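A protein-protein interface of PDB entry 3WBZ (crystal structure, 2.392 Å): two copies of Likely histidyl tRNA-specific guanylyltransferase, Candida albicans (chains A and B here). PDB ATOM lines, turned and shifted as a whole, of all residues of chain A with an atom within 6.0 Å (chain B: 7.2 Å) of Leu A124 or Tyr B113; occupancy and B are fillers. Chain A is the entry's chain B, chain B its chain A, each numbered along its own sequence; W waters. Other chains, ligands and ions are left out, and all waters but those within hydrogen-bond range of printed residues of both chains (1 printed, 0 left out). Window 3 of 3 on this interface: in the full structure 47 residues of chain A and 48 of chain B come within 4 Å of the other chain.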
ATOM      1  N   PHE A  39       1.026 -18.466 -37.623  1.00  0.00           N
ATOM      2  CA  PHE A  39       1.774 -17.227 -37.681  1.00  0.00           C
ATOM      3  C   PHE A  39       1.386 -16.482 -38.941  1.00  0.00           C
ATOM      4  O   PHE A  39       1.127 -15.292 -38.906  1.00  0.00           O
ATOM      5  CB  PHE A  39       3.299 -17.503 -37.641  1.00  0.00           C
ATOM      6  CG  PHE A  39       4.167 -16.255 -37.652  1.00  0.00           C
ATOM      7  CD1 PHE A  39       4.574 -15.665 -36.460  1.00  0.00           C
ATOM      8  CD2 PHE A  39       4.601 -15.694 -38.844  1.00  0.00           C
ATOM      9  CE1 PHE A  39       5.379 -14.540 -36.461  1.00  0.00           C
ATOM     10  CE2 PHE A  39       5.404 -14.551 -38.848  1.00  0.00           C
ATOM     11  CZ  PHE A  39       5.788 -13.979 -37.655  1.00  0.00           C
ATOM     12  N   PHE A  42      -2.316 -15.118 -38.632  1.00  0.00           N
ATOM     13  CA  PHE A  42      -2.410 -13.973 -37.731  1.00  0.00           C
ATOM     14  C   PHE A  42      -1.907 -12.665 -38.387  1.00  0.00           C
ATOM     15  O   PHE A  42      -2.514 -11.603 -38.226  1.00  0.00           O
ATOM     16  CB  PHE A  42      -1.632 -14.239 -36.450  1.00  0.00           C
ATOM     17  CG  PHE A  42      -1.814 -13.184 -35.407  1.00  0.00           C
ATOM     18  CD1 PHE A  42      -2.904 -13.218 -34.547  1.00  0.00           C
ATOM     19  CD2 PHE A  42      -0.899 -12.153 -35.280  1.00  0.00           C
ATOM     20  CE1 PHE A  42      -3.075 -12.240 -33.573  1.00  0.00           C
ATOM     21  CE2 PHE A  42      -1.075 -11.165 -34.318  1.00  0.00           C
ATOM     22  CZ  PHE A  42      -2.163 -11.209 -33.467  1.00  0.00           C
ATOM     23  N   TYR A  43      -0.822 -12.747 -39.149  1.00  0.00           N
ATOM     24  CA  TYR A  43      -0.272 -11.548 -39.747  1.00  0.00           C
ATOM     25  C   TYR A  43      -0.763 -11.378 -41.185  1.00  0.00           C
ATOM     26  O   TYR A  43      -0.248 -10.546 -41.937  1.00  0.00           O
ATOM     27  CB  TYR A  43       1.259 -11.553 -39.668  1.00  0.00           C
ATOM     28  CG  TYR A  43       1.714 -11.476 -38.241  1.00  0.00           C
ATOM     29  CD1 TYR A  43       1.503 -10.321 -37.496  1.00  0.00           C
ATOM     30  CD2 TYR A  43       2.348 -12.562 -37.624  1.00  0.00           C
ATOM     31  CE1 TYR A  43       1.897 -10.245 -36.184  1.00  0.00           C
ATOM     32  CE2 TYR A  43       2.742 -12.500 -36.311  1.00  0.00           C
ATOM     33  CZ  TYR A  43       2.528 -11.345 -35.592  1.00  0.00           C
ATOM     34  OH  TYR A  43       2.923 -11.287 -34.277  1.00  0.00           O
ATOM     35  N   TYR A 111      14.949 -12.542 -37.555  1.00  0.00           N
ATOM     36  CA  TYR A 111      13.631 -12.469 -38.154  1.00  0.00           C
ATOM     37  C   TYR A 111      12.814 -11.349 -37.511  1.00  0.00           C
ATOM     38  O   TYR A 111      12.214 -10.550 -38.225  1.00  0.00           O
ATOM     39  CB  TYR A 111      12.874 -13.802 -38.006  1.00  0.00           C
ATOM     40  CG  TYR A 111      11.630 -13.929 -38.886  1.00  0.00           C
ATOM     41  CD1 TYR A 111      10.447 -13.246 -38.578  1.00  0.00           C
ATOM     42  CD2 TYR A 111      11.634 -14.749 -40.003  1.00  0.00           C
ATOM     43  CE1 TYR A 111       9.316 -13.366 -39.376  1.00  0.00           C
ATOM     44  CE2 TYR A 111      10.517 -14.890 -40.799  1.00  0.00           C
ATOM     45  CZ  TYR A 111       9.360 -14.200 -40.488  1.00  0.00           C
ATOM     46  OH  TYR A 111       8.251 -14.349 -41.300  1.00  0.00           O
ATOM     47  N   MET A 112      12.798 -11.299 -36.174  1.00  0.00           N
ATOM     48  CA  MET A 112      12.090 -10.245 -35.451  1.00  0.00           C
ATOM     49  C   MET A 112      12.613  -8.859 -35.808  1.00  0.00           C
ATOM     50  O   MET A 112      11.828  -7.911 -35.942  1.00  0.00           O
ATOM     51  CB  MET A 112      12.196 -10.419 -33.933  1.00  0.00           C
ATOM     52  CG  MET A 112      11.137 -11.302 -33.348  1.00  0.00           C
ATOM     53  SD  MET A 112      11.061 -11.177 -31.568  1.00  0.00           S
ATOM     54  CE  MET A 112      10.267  -9.593 -31.397  1.00  0.00           C
ATOM     55  N   TRP A 115      11.589  -8.137 -39.491  1.00  0.00           N
ATOM     56  CA  TRP A 115      10.150  -8.021 -39.602  1.00  0.00           C
ATOM     57  C   TRP A 115       9.699  -6.581 -39.422  1.00  0.00           C
ATOM     58  O   TRP A 115       8.911  -6.064 -40.201  1.00  0.00           O
ATOM     59  CB  TRP A 115       9.464  -8.893 -38.568  1.00  0.00           C
ATOM     60  CG  TRP A 115       7.977  -8.722 -38.543  1.00  0.00           C
ATOM     61  CD1 TRP A 115       7.277  -7.807 -37.825  1.00  0.00           C
ATOM     62  CD2 TRP A 115       7.012  -9.470 -39.294  1.00  0.00           C
ATOM     63  NE1 TRP A 115       5.938  -7.947 -38.061  1.00  0.00           N
ATOM     64  CE2 TRP A 115       5.744  -8.960 -38.964  1.00  0.00           C
ATOM     65  CE3 TRP A 115       7.100 -10.528 -40.207  1.00  0.00           C
ATOM     66  CZ2 TRP A 115       4.558  -9.461 -39.520  1.00  0.00           C
ATOM     67  CZ3 TRP A 115       5.927 -11.037 -40.757  1.00  0.00           C
ATOM     68  CH2 TRP A 115       4.667 -10.497 -40.411  1.00  0.00           C
ATOM     69  N   SER A 116      10.252  -5.929 -38.414  1.00  0.00           N
ATOM     70  CA  SER A 116       9.883  -4.562 -38.108  1.00  0.00           C
ATOM     71  C   SER A 116      10.294  -3.585 -39.221  1.00  0.00           C
ATOM     72  O   SER A 116       9.689  -2.534 -39.336  1.00  0.00           O
ATOM     73  CB  SER A 116      10.436  -4.186 -36.718  1.00  0.00           C
ATOM     74  OG  SER A 116      11.840  -4.352 -36.597  1.00  0.00           O
ATOM     75  N   LYS A 122       2.413  -4.008 -39.155  1.00  0.00           N
ATOM     76  CA  LYS A 122       1.969  -5.215 -38.482  1.00  0.00           C
ATOM     77  C   LYS A 122       2.889  -5.511 -37.313  1.00  0.00           C
ATOM     78  O   LYS A 122       3.713  -6.416 -37.397  1.00  0.00           O
ATOM     79  CB  LYS A 122       1.951  -6.386 -39.462  1.00  0.00           C
ATOM     80  CG  LYS A 122       0.838  -6.321 -40.481  1.00  0.00           C
ATOM     81  CD  LYS A 122       0.956  -7.408 -41.535  1.00  0.00           C
ATOM     82  CE  LYS A 122      -0.218  -7.362 -42.513  1.00  0.00           C
ATOM     83  NZ  LYS A 122      -0.125  -8.381 -43.607  1.00  0.00           N
ATOM     84  N   PRO A 123       2.764  -4.735 -36.223  1.00  0.00           N
ATOM     85  CA  PRO A 123       3.622  -4.973 -35.063  1.00  0.00           C
ATOM     86  C   PRO A 123       3.416  -6.377 -34.498  1.00  0.00           C
ATOM     87  O   PRO A 123       2.326  -6.929 -34.568  1.00  0.00           O
ATOM     88  CB  PRO A 123       3.184  -3.890 -34.069  1.00  0.00           C
ATOM     89  CG  PRO A 123       1.803  -3.536 -34.479  1.00  0.00           C
ATOM     90  CD  PRO A 123       1.790  -3.660 -35.970  1.00  0.00           C
ATOM     91  N   LEU A 124       4.485  -6.959 -33.983  1.00  0.00           N
ATOM     92  CA  LEU A 124       4.435  -8.312 -33.487  1.00  0.00           C
ATOM     93  C   LEU A 124       3.687  -8.378 -32.163  1.00  0.00           C
ATOM     94  O   LEU A 124       3.861  -7.540 -31.298  1.00  0.00           O
ATOM     95  CB  LEU A 124       5.859  -8.846 -33.356  1.00  0.00           C
ATOM     96  CG  LEU A 124       6.487  -9.041 -34.733  1.00  0.00           C
ATOM     97  CD1 LEU A 124       7.998  -9.235 -34.673  1.00  0.00           C
ATOM     98  CD2 LEU A 124       5.818 -10.216 -35.412  1.00  0.00           C
ATOM     99  N   HIS A 125       2.835  -9.381 -32.045  1.00  0.00           N
ATOM    100  CA  HIS A 125       2.060  -9.660 -30.849  1.00  0.00           C
ATOM    101  C   HIS A 125       2.779 -10.668 -29.962  1.00  0.00           C
ATOM    102  O   HIS A 125       3.383 -11.614 -30.469  1.00  0.00           O
ATOM    103  CB  HIS A 125       0.689 -10.184 -31.265  1.00  0.00           C
ATOM    104  CG  HIS A 125      -0.287 -10.323 -30.144  1.00  0.00           C
ATOM    105  ND1 HIS A 125      -0.305 -11.418 -29.305  1.00  0.00           N
ATOM    106  CD2 HIS A 125      -1.295  -9.516 -29.735  1.00  0.00           C
ATOM    107  CE1 HIS A 125      -1.279 -11.275 -28.424  1.00  0.00           C
ATOM    108  NE2 HIS A 125      -1.896 -10.131 -28.665  1.00  0.00           N
ATOM    109  N   ILE A 126       2.674 -10.496 -28.647  1.00  0.00           N
ATOM    110  CA  ILE A 126       3.422 -11.314 -27.690  1.00  0.00           C
ATOM    111  C   ILE A 126       3.124 -12.809 -27.838  1.00  0.00           C
ATOM    112  O   ILE A 126       3.979 -13.654 -27.550  1.00  0.00           O
ATOM    113  CB  ILE A 126       3.100 -10.866 -26.230  1.00  0.00           C
ATOM    114  CG1 ILE A 126       3.926 -11.634 -25.196  1.00  0.00           C
ATOM    115  CG2 ILE A 126       1.669 -11.164 -25.904  1.00  0.00           C
ATOM    116  CD1 ILE A 126       5.397 -11.643 -25.449  1.00  0.00           C
ATOM    117  N   HIS A 128       2.450 -14.258 -30.735  1.00  0.00           N
ATOM    118  CA  HIS A 128       2.756 -14.688 -32.091  1.00  0.00           C
ATOM    119  C   HIS A 128       4.123 -14.194 -32.558  1.00  0.00           C
ATOM    120  O   HIS A 128       4.249 -13.484 -33.565  1.00  0.00           O
ATOM    121  CB  HIS A 128       1.655 -14.214 -33.043  1.00  0.00           C
ATOM    122  CG  HIS A 128       0.297 -14.707 -32.661  1.00  0.00           C
ATOM    123  ND1 HIS A 128      -0.567 -13.972 -31.873  1.00  0.00           N
ATOM    124  CD2 HIS A 128      -0.315 -15.897 -32.874  1.00  0.00           C
ATOM    125  CE1 HIS A 128      -1.670 -14.666 -31.670  1.00  0.00           C
ATOM    126  NE2 HIS A 128      -1.542 -15.842 -32.263  1.00  0.00           N
ATOM    127  N   LEU A 129       5.159 -14.563 -31.815  1.00  0.00           N
ATOM    128  CA  LEU A 129       6.521 -14.236 -32.219  1.00  0.00           C
ATOM    129  C   LEU A 129       7.089 -15.285 -33.165  1.00  0.00           C
ATOM    130  O   LEU A 129       6.673 -16.423 -33.136  1.00  0.00           O
ATOM    131  CB  LEU A 129       7.395 -14.086 -30.985  1.00  0.00           C
ATOM    132  CG  LEU A 129       6.797 -12.989 -30.102  1.00  0.00           C
ATOM    133  CD1 LEU A 129       7.633 -12.796 -28.869  1.00  0.00           C
ATOM    134  CD2 LEU A 129       6.657 -11.686 -30.887  1.00  0.00           C
ATOM    135  N   PRO A 130       8.032 -14.898 -34.036  1.00  0.00           N
ATOM    136  CA  PRO A 130       8.603 -15.915 -34.933  1.00  0.00           C
ATOM    137  C   PRO A 130       9.678 -16.794 -34.254  1.00  0.00           C
ATOM    138  O   PRO A 130      10.767 -16.308 -33.939  1.00  0.00           O
ATOM    139  CB  PRO A 130       9.234 -15.083 -36.043  1.00  0.00           C
ATOM    140  CG  PRO A 130       9.644 -13.803 -35.341  1.00  0.00           C
ATOM    141  CD  PRO A 130       8.588 -13.554 -34.286  1.00  0.00           C
ATOM    142  N   VAL B  56      13.032  -8.011 -17.697  1.00  0.00           N
ATOM    143  CA  VAL B  56      12.909  -8.583 -19.023  1.00  0.00           C
ATOM    144  C   VAL B  56      13.103 -10.110 -19.009  1.00  0.00           C
ATOM    145  O   VAL B  56      12.314 -10.847 -19.619  1.00  0.00           O
ATOM    146  CB  VAL B  56      13.922  -7.977 -19.981  1.00  0.00           C
ATOM    147  CG1 VAL B  56      13.851  -8.687 -21.330  1.00  0.00           C
ATOM    148  CG2 VAL B  56      13.622  -6.520 -20.166  1.00  0.00           C
ATOM    149  N   MET B 107      13.072 -18.006 -25.530  1.00  0.00           N
ATOM    150  CA  MET B 107      13.649 -17.034 -24.612  1.00  0.00           C
ATOM    151  C   MET B 107      14.190 -15.849 -25.398  1.00  0.00           C
ATOM    152  O   MET B 107      14.035 -14.707 -24.974  1.00  0.00           O
ATOM    153  CB  MET B 107      14.769 -17.659 -23.765  1.00  0.00           C
ATOM    154  CG  MET B 107      14.271 -18.510 -22.595  1.00  0.00           C
ATOM    155  SD  MET B 107      13.247 -17.565 -21.449  1.00  0.00           S
ATOM    156  CE  MET B 107      14.490 -16.423 -20.823  1.00  0.00           C
ATOM    157  N   SER B 108      14.787 -16.124 -26.559  1.00  0.00           N
ATOM    158  CA  SER B 108      15.351 -15.071 -27.399  1.00  0.00           C
ATOM    159  C   SER B 108      14.304 -14.067 -27.869  1.00  0.00           C
ATOM    160  O   SER B 108      14.519 -12.863 -27.772  1.00  0.00           O
ATOM    161  CB  SER B 108      16.034 -15.665 -28.620  1.00  0.00           C
ATOM    162  OG  SER B 108      17.185 -16.392 -28.254  1.00  0.00           O
ATOM    163  N   THR B 109      13.187 -14.579 -28.386  1.00  0.00           N
ATOM    164  CA  THR B 109      12.153 -13.720 -28.961  1.00  0.00           C
ATOM    165  C   THR B 109      11.346 -13.035 -27.875  1.00  0.00           C
ATOM    166  O   THR B 109      11.006 -11.861 -28.018  1.00  0.00           O
ATOM    167  CB  THR B 109      11.212 -14.494 -29.929  1.00  0.00           C
ATOM    168  OG1 THR B 109      10.596 -15.624 -29.284  1.00  0.00           O
ATOM    169  CG2 THR B 109      11.982 -14.958 -31.143  1.00  0.00           C
ATOM    170  N   TYR B 110      11.054 -13.749 -26.788  1.00  0.00           N
ATOM    171  CA  TYR B 110      10.401 -13.136 -25.636  1.00  0.00           C
ATOM    172  C   TYR B 110      11.288 -12.049 -25.070  1.00  0.00           C
ATOM    173  O   TYR B 110      10.791 -11.003 -24.680  1.00  0.00           O
ATOM    174  CB  TYR B 110      10.073 -14.159 -24.538  1.00  0.00           C
ATOM    175  CG  TYR B 110       8.864 -15.036 -24.797  1.00  0.00           C
ATOM    176  CD1 TYR B 110       7.731 -14.546 -25.464  1.00  0.00           C
ATOM    177  CD2 TYR B 110       8.849 -16.350 -24.377  1.00  0.00           C
ATOM    178  CE1 TYR B 110       6.633 -15.358 -25.699  1.00  0.00           C
ATOM    179  CE2 TYR B 110       7.761 -17.169 -24.609  1.00  0.00           C
ATOM    180  CZ  TYR B 110       6.657 -16.674 -25.259  1.00  0.00           C
ATOM    181  OH  TYR B 110       5.588 -17.513 -25.467  1.00  0.00           O
ATOM    182  N   TYR B 111      12.605 -12.280 -25.045  1.00  0.00           N
ATOM    183  CA  TYR B 111      13.526 -11.259 -24.533  1.00  0.00           C
ATOM    184  C   TYR B 111      13.436  -9.997 -25.402  1.00  0.00           C
ATOM    185  O   TYR B 111      13.292  -8.900 -24.872  1.00  0.00           O
ATOM    186  CB  TYR B 111      14.986 -11.769 -24.490  1.00  0.00           C
ATOM    187  CG  TYR B 111      15.926 -10.872 -23.683  1.00  0.00           C
ATOM    188  CD1 TYR B 111      16.378  -9.650 -24.197  1.00  0.00           C
ATOM    189  CD2 TYR B 111      16.336 -11.227 -22.407  1.00  0.00           C
ATOM    190  CE1 TYR B 111      17.226  -8.815 -23.459  1.00  0.00           C
ATOM    191  CE2 TYR B 111      17.172 -10.401 -21.664  1.00  0.00           C
ATOM    192  CZ  TYR B 111      17.617  -9.197 -22.197  1.00  0.00           C
ATOM    193  OH  TYR B 111      18.456  -8.384 -21.465  1.00  0.00           O
ATOM    194  N   MET B 112      13.486 -10.166 -26.726  1.00  0.00           N
ATOM    195  CA  MET B 112      13.354  -9.043 -27.662  1.00  0.00           C
ATOM    196  C   MET B 112      12.033  -8.297 -27.509  1.00  0.00           C
ATOM    197  O   MET B 112      12.012  -7.066 -27.531  1.00  0.00           O
ATOM    198  CB  MET B 112      13.482  -9.516 -29.107  1.00  0.00           C
ATOM    199  CG  MET B 112      14.878  -9.562 -29.578  1.00  0.00           C
ATOM    200  SD  MET B 112      15.052  -9.906 -31.327  1.00  0.00           S
ATOM    201  CE  MET B 112      14.633  -8.348 -32.112  1.00  0.00           C
ATOM    202  N   TYR B 113      10.943  -9.034 -27.341  1.00  0.00           N
ATOM    203  CA  TYR B 113       9.653  -8.385 -27.168  1.00  0.00           C
ATOM    204  C   TYR B 113       9.655  -7.496 -25.933  1.00  0.00           C
ATOM    205  O   TYR B 113       9.418  -6.301 -26.020  1.00  0.00           O
ATOM    206  CB  TYR B 113       8.518  -9.407 -27.051  1.00  0.00           C
ATOM    207  CG  TYR B 113       7.191  -8.728 -26.852  1.00  0.00           C
ATOM    208  CD1 TYR B 113       6.471  -8.248 -27.937  1.00  0.00           C
ATOM    209  CD2 TYR B 113       6.666  -8.540 -25.581  1.00  0.00           C
ATOM    210  CE1 TYR B 113       5.274  -7.616 -27.762  1.00  0.00           C
ATOM    211  CE2 TYR B 113       5.463  -7.908 -25.398  1.00  0.00           C
ATOM    212  CZ  TYR B 113       4.769  -7.443 -26.486  1.00  0.00           C
ATOM    213  OH  TYR B 113       3.554  -6.801 -26.295  1.00  0.00           O
ATOM    214  N   PHE B 114       9.998  -8.085 -24.799  1.00  0.00           N
ATOM    215  CA  PHE B 114       9.936  -7.396 -23.527  1.00  0.00           C
ATOM    216  C   PHE B 114      10.998  -6.314 -23.393  1.00  0.00           C
ATOM    217  O   PHE B 114      10.826  -5.384 -22.616  1.00  0.00           O
ATOM    218  CB  PHE B 114      10.049  -8.393 -22.376  1.00  0.00           C
ATOM    219  CG  PHE B 114       8.771  -9.152 -22.115  1.00  0.00           C
ATOM    220  CD1 PHE B 114       7.626  -8.481 -21.693  1.00  0.00           C
ATOM    221  CD2 PHE B 114       8.715 -10.535 -22.294  1.00  0.00           C
ATOM    222  CE1 PHE B 114       6.446  -9.172 -21.455  1.00  0.00           C
ATOM    223  CE2 PHE B 114       7.528 -11.241 -22.057  1.00  0.00           C
ATOM    224  CZ  PHE B 114       6.393 -10.564 -21.632  1.00  0.00           C
ATOM    225  N   TRP B 115      12.104  -6.452 -24.114  1.00  0.00           N
ATOM    226  CA  TRP B 115      13.109  -5.406 -24.135  1.00  0.00           C
ATOM    227  C   TRP B 115      12.503  -4.130 -24.774  1.00  0.00           C
ATOM    228  O   TRP B 115      12.725  -3.029 -24.293  1.00  0.00           O
ATOM    229  CB  TRP B 115      14.382  -5.859 -24.872  1.00  0.00           C
ATOM    230  CG  TRP B 115      15.419  -4.755 -24.967  1.00  0.00           C
ATOM    231  CD1 TRP B 115      15.490  -3.775 -25.928  1.00  0.00           C
ATOM    232  CD2 TRP B 115      16.513  -4.511 -24.065  1.00  0.00           C
ATOM    233  NE1 TRP B 115      16.556  -2.946 -25.677  1.00  0.00           N
ATOM    234  CE2 TRP B 115      17.202  -3.375 -24.547  1.00  0.00           C
ATOM    235  CE3 TRP B 115      16.976  -5.143 -22.907  1.00  0.00           C
ATOM    236  CZ2 TRP B 115      18.327  -2.854 -23.902  1.00  0.00           C
ATOM    237  CZ3 TRP B 115      18.103  -4.630 -22.270  1.00  0.00           C
ATOM    238  CH2 TRP B 115      18.761  -3.488 -22.772  1.00  0.00           C
ATOM    239  N   SER B 116      11.747  -4.277 -25.858  1.00  0.00           N
ATOM    240  CA  SER B 116      11.173  -3.099 -26.502  1.00  0.00           C
ATOM    241  C   SER B 116      10.123  -2.438 -25.603  1.00  0.00           C
ATOM    242  O   SER B 116       9.850  -1.250 -25.743  1.00  0.00           O
ATOM    243  CB  SER B 116      10.558  -3.449 -27.859  1.00  0.00           C
ATOM    244  OG  SER B 116       9.488  -4.362 -27.721  1.00  0.00           O
ATOM    245  N   GLN B 117       9.549  -3.203 -24.676  1.00  0.00           N
ATOM    246  CA  GLN B 117       8.591  -2.651 -23.704  1.00  0.00           C
ATOM    247  C   GLN B 117       9.263  -1.911 -22.549  1.00  0.00           C
ATOM    248  O   GLN B 117       8.827  -0.827 -22.171  1.00  0.00           O
ATOM    249  CB  GLN B 117       7.701  -3.755 -23.143  1.00  0.00           C
ATOM    250  CG  GLN B 117       6.888  -4.484 -24.193  1.00  0.00           C
ATOM    251  CD  GLN B 117       5.999  -3.562 -24.999  1.00  0.00           C
ATOM    252  OE1 GLN B 117       6.367  -3.118 -26.091  1.00  0.00           O
ATOM    253  NE2 GLN B 117       4.821  -3.255 -24.459  1.00  0.00           N
ATOM    254  N   TYR B 118      10.304  -2.521 -21.974  1.00  0.00           N
ATOM    255  CA  TYR B 118      11.004  -1.965 -20.813  1.00  0.00           C
ATOM    256  C   TYR B 118      12.073  -0.928 -21.212  1.00  0.00           C
ATOM    257  O   TYR B 118      12.381  -0.022 -20.444  1.00  0.00           O
ATOM    258  CB  TYR B 118      11.668  -3.091 -20.000  1.00  0.00           C
ATOM    259  CG  TYR B 118      10.719  -3.962 -19.196  1.00  0.00           C
ATOM    260  CD1 TYR B 118      10.081  -5.051 -19.772  1.00  0.00           C
ATOM    261  CD2 TYR B 118      10.463  -3.691 -17.850  1.00  0.00           C
ATOM    262  CE1 TYR B 118       9.207  -5.844 -19.041  1.00  0.00           C
ATOM    263  CE2 TYR B 118       9.596  -4.478 -17.113  1.00  0.00           C
ATOM    264  CZ  TYR B 118       8.973  -5.555 -17.720  1.00  0.00           C
ATOM    265  OH  TYR B 118       8.116  -6.338 -16.996  1.00  0.00           O
ATOM    266  N   PHE B 119      12.627  -1.043 -22.413  1.00  0.00           N
ATOM    267  CA  PHE B 119      13.630  -0.084 -22.875  1.00  0.00           C
ATOM    268  C   PHE B 119      13.301   0.519 -24.237  1.00  0.00           C
ATOM    269  O   PHE B 119      14.037   0.296 -25.200  1.00  0.00           O
ATOM    270  CB  PHE B 119      15.007  -0.732 -22.975  1.00  0.00           C
ATOM    271  CG  PHE B 119      15.572  -1.206 -21.665  1.00  0.00           C
ATOM    272  CD1 PHE B 119      16.279  -0.342 -20.841  1.00  0.00           C
ATOM    273  CD2 PHE B 119      15.420  -2.527 -21.273  1.00  0.00           C
ATOM    274  CE1 PHE B 119      16.820  -0.785 -19.653  1.00  0.00           C
ATOM    275  CE2 PHE B 119      15.945  -2.967 -20.088  1.00  0.00           C
ATOM    276  CZ  PHE B 119      16.655  -2.092 -19.273  1.00  0.00           C
ATOM    277  N   LEU B 124      17.158  -2.134 -30.150  1.00  0.00           N
ATOM    278  CA  LEU B 124      18.213  -3.121 -30.326  1.00  0.00           C
ATOM    279  C   LEU B 124      18.955  -2.914 -31.644  1.00  0.00           C
ATOM    280  O   LEU B 124      18.358  -2.647 -32.688  1.00  0.00           O
ATOM    281  CB  LEU B 124      17.647  -4.543 -30.268  1.00  0.00           C
ATOM    282  CG  LEU B 124      17.098  -5.053 -28.929  1.00  0.00           C
ATOM    283  CD1 LEU B 124      16.364  -6.380 -29.123  1.00  0.00           C
ATOM    284  CD2 LEU B 124      18.161  -5.165 -27.851  1.00  0.00           C
ATOM    285  N   PRO B 130      19.835 -10.245 -28.499  1.00  0.00           N
ATOM    286  CA  PRO B 130      19.960 -11.166 -27.368  1.00  0.00           C
ATOM    287  C   PRO B 130      19.788 -12.626 -27.786  1.00  0.00           C
ATOM    288  O   PRO B 130      18.689 -13.045 -28.152  1.00  0.00           O
ATOM    289  CB  PRO B 130      18.826 -10.739 -26.438  1.00  0.00           C
ATOM    290  CG  PRO B 130      17.775 -10.218 -27.380  1.00  0.00           C
ATOM    291  CD  PRO B 130      18.528  -9.565 -28.515  1.00  0.00           C
HETATM  292  O   HOH W   1       1.700  -8.207 -27.793  1.00  0.00           O
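Met B112 touches its own counterpart, Met A112.
Positions printed for both chains: 111, 112, 115, 116, 124 and 130.
Of the 9 pairs that touch across the chains among the printed residues, 1 has its exchanged pair printed and touching as well.
The side-chain sulfur of Met A112 lies close to the backbone carbonyl oxygen of Thr B109, at 3.6 Å.
The backbone carbonyl oxygen (O) of Tyr B113 is in hydrogen-bond range of the side-chain hydroxyl (OG) of Ser B116, at 2.6 Å.
Of chain B, only Tyr B113 (3.8 Å) comes within 4 Å of Leu A124.
Tyr B113 touches just these residues of chain A: Leu A124 (3.8 Å), Ile A126 (3.4 Å) and Leu A129 (3.9 Å).
Printed residues of chain A within 4 Å of Tyr B110: Ile A126 (3.7 Å) and Leu A129 (3.8 Å).
Printed residues of chain B within 4 Å of Pro A130: Thr B109 (3.3 Å).
Of the printed residues of chain B, Met A112 touches Thr B109 (3.6 Å) and Met B112 (3.7 Å).
Of the printed residues of chain B, Leu A129 touches Thr B109 (3.6 Å), Tyr B110 (3.8 Å) and Tyr B113 (3.9 Å).
Of the printed residues of chain A, Thr B109 touches Met A112, Leu A129 and Pro A130.
His A125 touches none of the printed residues of chain B.
Ser A116 touches none of the printed residues of chain B.
Hydrophobic or aromatic side chains of chain B within 4 Å of the printed part of chain A: Tyr B110, Met B112 and Tyr B113.
Among the printed residues, 9 pairs touch across the chains.
Among the printed residues, no Asp or Glu carboxylate lies within 4 Å of a Lys or Arg side-chain nitrogen of the other chain.
CB of Met A112 touches CE of Met B112, at 3.7 Å.
O of Leu A124 touches CE1 of Tyr B113, at 3.8 Å.
Tyr B110 touches Ile A126 (CE1 to O, 3.7 Å).
Tyr B113 touches Ile A126 (CD2 to CD1, 3.4 Å).
CD1 of Leu A129 touches O of Thr B109, 3.6 Å away.
Tyr B110 touches Leu A129.
CB of Tyr B113 touches CD1 of Leu A129, 3.9 Å away.
O of Pro A130 touches CG2 of Thr B109, 3.3 Å away.
Water W1 bridges N of Ile A126 (2.6 Å) and OH of Tyr B113 (2.8 Å).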
